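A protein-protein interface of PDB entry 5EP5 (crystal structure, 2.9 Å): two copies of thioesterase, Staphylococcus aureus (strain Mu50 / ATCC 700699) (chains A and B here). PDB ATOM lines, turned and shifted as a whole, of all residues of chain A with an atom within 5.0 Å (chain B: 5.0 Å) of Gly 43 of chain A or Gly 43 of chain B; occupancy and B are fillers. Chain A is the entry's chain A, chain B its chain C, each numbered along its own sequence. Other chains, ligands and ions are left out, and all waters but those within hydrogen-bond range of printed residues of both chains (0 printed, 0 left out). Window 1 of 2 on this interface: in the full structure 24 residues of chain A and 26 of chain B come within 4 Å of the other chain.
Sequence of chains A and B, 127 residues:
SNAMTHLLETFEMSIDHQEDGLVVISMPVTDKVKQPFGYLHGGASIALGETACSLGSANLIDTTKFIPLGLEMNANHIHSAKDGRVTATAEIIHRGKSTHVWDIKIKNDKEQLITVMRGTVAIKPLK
His 41 of chain A touches Glu 50 of chain B, but with the chains exchanged Glu 50 of chain A does not touch His 41 of chain B (4.2 Å).
Gly 43 of chain B touches its own counterpart, Gly 43 of chain A.
Gly 43 of chain A touches Ala 47 of chain B, and with the chains exchanged Ala 47 of chain A touches Gly 43 of chain B.
Ile 46 of chain B touches its own counterpart, Ile 46 of chain A.
9 positions are printed for both chains.
Of the 7 pairs that touch across the chains among the printed residues, 6 have their exchanged pair printed and touching as well.
Printed residues of chain B within 4 Å of Ala 47 of chain A: His 41 and Gly 43.
Glu 50 of chain A touches none of the printed residues of chain B.
Gly 43 of chain B touches just these residues of chain A: Gly 43 (3.98 Å) and Ala 47 (3.8 Å).
Of the printed residues of chain A, Ile 46 of chain B touches Ile 46.
The nearest residue of chain B that does not touch Gly 43 of chain A is Glu 50 of chain B (4.4 Å).
The nearest printed residue of chain B that does not touch His 41 of chain A is Ile 46 of chain B (5.8 Å).
Of the 9 printed residues of chain A, 4 touch a printed residue of chain B.
Printed residues of chain A that touch a printed residue of chain B: His 41, Gly 43, Ile 46 and Ala 47.
Hydrophobic or aromatic side chains of chain A within 4 Å of the printed part of chain B: His 41, Ile 46 and Ala 47.
Of the 9 printed residues of chain B, 5 touch a printed residue of chain A.
Along chain B the printed residues that touch a printed residue of chain A span positions 41 to 50.
Among the printed residues, no Asp or Glu carboxylate lies within 4 Å of a Lys or Arg side-chain nitrogen of the other chain.
A ring nitrogen (ND1) of His 41 of chain A lies within hydrogen-bond range of the backbone NH of Gly 43 of chain A, at 3.0 Å.
A ring nitrogen (ND1) of His 41 of chain B sits at hydrogen-bond distance from the backbone NH (N) of Gly 43 of chain B, 3.0 Å away.
His 41 of chain A touches Ala 47 of chain B (CE1 to O, 3.6 Å).
His 41 of chain A touches Glu 50 of chain B (CE1 to CB, 3.9 Å).
O of Gly 43 of chain A touches O of Gly 43 of chain B, at 3.98 Å.
Ala 47 of chain B touches Gly 43 of chain A.
CG2 of Ile 46 of chain A touches CG2 of Ile 46 of chain B, 3.9 Å away.
Ala 47 of chain A touches His 41 of chain B (O to CE1, 3.6 Å).
Ala 47 of chain A touches Gly 43 of chain B (CA to CA, 3.8 Å).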
ATOM      1  N   HIS A  41      11.927  -4.974 -34.653  1.00  0.00           N
ATOM      2  CA  HIS A  41      11.653  -4.738 -33.227  1.00  0.00           C
ATOM      3  C   HIS A  41      10.562  -3.676 -33.144  1.00  0.00           C
ATOM      4  O   HIS A  41      10.625  -2.669 -33.843  1.00  0.00           O
ATOM      5  CB  HIS A  41      12.952  -4.245 -32.564  1.00  0.00           C
ATOM      6  CG  HIS A  41      12.941  -4.222 -31.059  1.00  0.00           C
ATOM      7  ND1 HIS A  41      12.143  -3.377 -30.328  1.00  0.00           N
ATOM      8  CD2 HIS A  41      13.708  -4.877 -30.153  1.00  0.00           C
ATOM      9  CE1 HIS A  41      12.378  -3.538 -29.040  1.00  0.00           C
ATOM     10  NE2 HIS A  41      13.329  -4.443 -28.905  1.00  0.00           N
ATOM     11  N   GLY A  42       9.562  -3.896 -32.298  1.00  0.00           N
ATOM     12  CA  GLY A  42       8.440  -2.952 -32.162  1.00  0.00           C
ATOM     13  C   GLY A  42       8.916  -1.558 -31.800  1.00  0.00           C
ATOM     14  O   GLY A  42       8.447  -0.555 -32.329  1.00  0.00           O
ATOM     15  N   GLY A  43       9.807  -1.517 -30.824  1.00  0.00           N
ATOM     16  CA  GLY A  43      10.529  -0.316 -30.444  1.00  0.00           C
ATOM     17  C   GLY A  43      11.244   0.448 -31.538  1.00  0.00           C
ATOM     18  O   GLY A  43      11.336   1.666 -31.472  1.00  0.00           O
ATOM     19  N   ALA A  44      11.782  -0.241 -32.532  1.00  0.00           N
ATOM     20  CA  ALA A  44      12.517   0.442 -33.595  1.00  0.00           C
ATOM     21  C   ALA A  44      11.534   1.157 -34.502  1.00  0.00           C
ATOM     22  O   ALA A  44      11.789   2.277 -34.947  1.00  0.00           O
ATOM     23  CB  ALA A  44      13.352  -0.543 -34.376  1.00  0.00           C
ATOM     24  N   SER A  45      10.408   0.492 -34.755  1.00  0.00           N
ATOM     25  CA  SER A  45       9.278   1.089 -35.461  1.00  0.00           C
ATOM     26  C   SER A  45       8.781   2.340 -34.730  1.00  0.00           C
ATOM     27  O   SER A  45       8.616   3.391 -35.323  1.00  0.00           O
ATOM     28  CB  SER A  45       8.154   0.048 -35.587  1.00  0.00           C
ATOM     29  OG  SER A  45       7.083   0.507 -36.385  1.00  0.00           O
ATOM     30  N   ILE A  46       8.582   2.230 -33.428  1.00  0.00           N
ATOM     31  CA  ILE A  46       8.151   3.365 -32.623  1.00  0.00           C
ATOM     32  C   ILE A  46       9.187   4.489 -32.704  1.00  0.00           C
ATOM     33  O   ILE A  46       8.829   5.637 -32.856  1.00  0.00           O
ATOM     34  CB  ILE A  46       7.884   2.934 -31.160  1.00  0.00           C
ATOM     35  CG1 ILE A  46       6.683   1.990 -31.121  1.00  0.00           C
ATOM     36  CG2 ILE A  46       7.627   4.123 -30.257  1.00  0.00           C
ATOM     37  CD1 ILE A  46       6.514   1.227 -29.829  1.00  0.00           C
ATOM     38  N   ALA A  47      10.466   4.154 -32.630  1.00  0.00           N
ATOM     39  CA  ALA A  47      11.517   5.153 -32.704  1.00  0.00           C
ATOM     40  C   ALA A  47      11.503   5.906 -34.053  1.00  0.00           C
ATOM     41  O   ALA A  47      11.708   7.115 -34.099  1.00  0.00           O
ATOM     42  CB  ALA A  47      12.865   4.496 -32.461  1.00  0.00           C
ATOM     43  N   GLU A  50       8.504   8.320 -33.744  1.00  0.00           N
ATOM     44  CA  GLU A  50       8.798   9.432 -32.869  1.00  0.00           C
ATOM     45  C   GLU A  50       9.732  10.393 -33.564  1.00  0.00           C
ATOM     46  O   GLU A  50       9.609  11.601 -33.421  1.00  0.00           O
ATOM     47  CB  GLU A  50       9.400   8.952 -31.572  1.00  0.00           C
ATOM     48  N   HIS A  77       0.862  -2.428 -32.582  1.00  0.00           N
ATOM     49  CA  HIS A  77       1.575  -3.227 -33.539  1.00  0.00           C
ATOM     50  C   HIS A  77       0.557  -4.135 -34.217  1.00  0.00           C
ATOM     51  O   HIS A  77      -0.157  -4.861 -33.537  1.00  0.00           O
ATOM     52  CB  HIS A  77       2.654  -4.019 -32.804  1.00  0.00           C
ATOM     53  CG  HIS A  77       3.719  -3.155 -32.202  1.00  0.00           C
ATOM     54  ND1 HIS A  77       4.408  -2.220 -32.942  1.00  0.00           N
ATOM     55  CD2 HIS A  77       4.210  -3.074 -30.941  1.00  0.00           C
ATOM     56  CE1 HIS A  77       5.275  -1.594 -32.164  1.00  0.00           C
ATOM     57  NE2 HIS A  77       5.175  -2.095 -30.944  1.00  0.00           N
ATOM     58  N   HIS B  41      17.131   9.928 -27.195  1.00  0.00           N
ATOM     59  CA  HIS B  41      15.953   9.896 -28.092  1.00  0.00           C
ATOM     60  C   HIS B  41      14.823   9.168 -27.384  1.00  0.00           C
ATOM     61  O   HIS B  41      15.049   8.139 -26.795  1.00  0.00           O
ATOM     62  CB  HIS B  41      16.339   9.182 -29.387  1.00  0.00           C
ATOM     63  CG  HIS B  41      15.394   9.373 -30.528  1.00  0.00           C
ATOM     64  ND1 HIS B  41      14.170   8.760 -30.567  1.00  0.00           N
ATOM     65  CD2 HIS B  41      15.535  10.003 -31.720  1.00  0.00           C
ATOM     66  CE1 HIS B  41      13.573   9.027 -31.714  1.00  0.00           C
ATOM     67  NE2 HIS B  41      14.380   9.788 -32.432  1.00  0.00           N
ATOM     68  N   GLY B  42      13.625   9.734 -27.411  1.00  0.00           N
ATOM     69  CA  GLY B  42      12.483   9.159 -26.724  1.00  0.00           C
ATOM     70  C   GLY B  42      12.184   7.770 -27.237  1.00  0.00           C
ATOM     71  O   GLY B  42      11.872   6.865 -26.465  1.00  0.00           O
ATOM     72  N   GLY B  43      12.228   7.618 -28.550  1.00  0.00           N
ATOM     73  CA  GLY B  43      12.164   6.310 -29.179  1.00  0.00           C
ATOM     74  C   GLY B  43      13.130   5.248 -28.688  1.00  0.00           C
ATOM     75  O   GLY B  43      12.769   4.055 -28.635  1.00  0.00           O
ATOM     76  N   ALA B  44      14.359   5.661 -28.370  1.00  0.00           N
ATOM     77  CA  ALA B  44      15.386   4.728 -27.903  1.00  0.00           C
ATOM     78  C   ALA B  44      15.032   4.235 -26.508  1.00  0.00           C
ATOM     79  O   ALA B  44      15.168   3.043 -26.202  1.00  0.00           O
ATOM     80  CB  ALA B  44      16.758   5.382 -27.898  1.00  0.00           C
ATOM     81  N   SER B  45      14.566   5.171 -25.681  1.00  0.00           N
ATOM     82  CA  SER B  45      14.061   4.861 -24.357  1.00  0.00           C
ATOM     83  C   SER B  45      12.875   3.880 -24.436  1.00  0.00           C
ATOM     84  O   SER B  45      12.847   2.841 -23.744  1.00  0.00           O
ATOM     85  CB  SER B  45      13.670   6.156 -23.628  1.00  0.00           C
ATOM     86  OG  SER B  45      13.323   5.910 -22.275  1.00  0.00           O
ATOM     87  N   ILE B  46      11.922   4.165 -25.316  1.00  0.00           N
ATOM     88  CA  ILE B  46      10.787   3.250 -25.492  1.00  0.00           C
ATOM     89  C   ILE B  46      11.274   1.863 -25.984  1.00  0.00           C
ATOM     90  O   ILE B  46      10.821   0.842 -25.491  1.00  0.00           O
ATOM     91  CB  ILE B  46       9.720   3.853 -26.429  1.00  0.00           C
ATOM     92  CG1 ILE B  46       9.131   5.115 -25.814  1.00  0.00           C
ATOM     93  CG2 ILE B  46       8.597   2.862 -26.715  1.00  0.00           C
ATOM     94  CD1 ILE B  46       8.386   5.974 -26.808  1.00  0.00           C
ATOM     95  N   ALA B  47      12.220   1.835 -26.924  1.00  0.00           N
ATOM     96  CA  ALA B  47      12.802   0.569 -27.385  1.00  0.00           C
ATOM     97  C   ALA B  47      13.476  -0.236 -26.264  1.00  0.00           C
ATOM     98  O   ALA B  47      13.389  -1.450 -26.236  1.00  0.00           O
ATOM     99  CB  ALA B  47      13.788   0.829 -28.508  1.00  0.00           C
ATOM    100  N   GLU B  50      10.518  -1.773 -24.354  1.00  0.00           N
ATOM    101  CA  GLU B  50       9.891  -2.834 -25.114  1.00  0.00           C
ATOM    102  C   GLU B  50      10.757  -4.086 -25.083  1.00  0.00           C
ATOM    103  O   GLU B  50      10.257  -5.210 -24.984  1.00  0.00           O
ATOM    104  CB  GLU B  50       9.629  -2.389 -26.543  1.00  0.00           C
ATOM    105  N   HIS B  77       7.075  10.608 -21.451  1.00  0.00           N
ATOM    106  CA  HIS B  77       8.408  11.115 -21.258  1.00  0.00           C
ATOM    107  C   HIS B  77       8.320  12.213 -20.195  1.00  0.00           C
ATOM    108  O   HIS B  77       7.514  13.131 -20.327  1.00  0.00           O
ATOM    109  CB  HIS B  77       8.923  11.653 -22.580  1.00  0.00           C
ATOM    110  CG  HIS B  77       9.097  10.604 -23.639  1.00  0.00           C
ATOM    111  ND1 HIS B  77       9.889   9.492 -23.452  1.00  0.00           N
ATOM    112  CD2 HIS B  77       8.625  10.519 -24.907  1.00  0.00           C
ATOM    113  CE1 HIS B  77       9.882   8.756 -24.550  1.00  0.00           C
ATOM    114  NE2 HIS B  77       9.129   9.363 -25.451  1.00  0.00           N
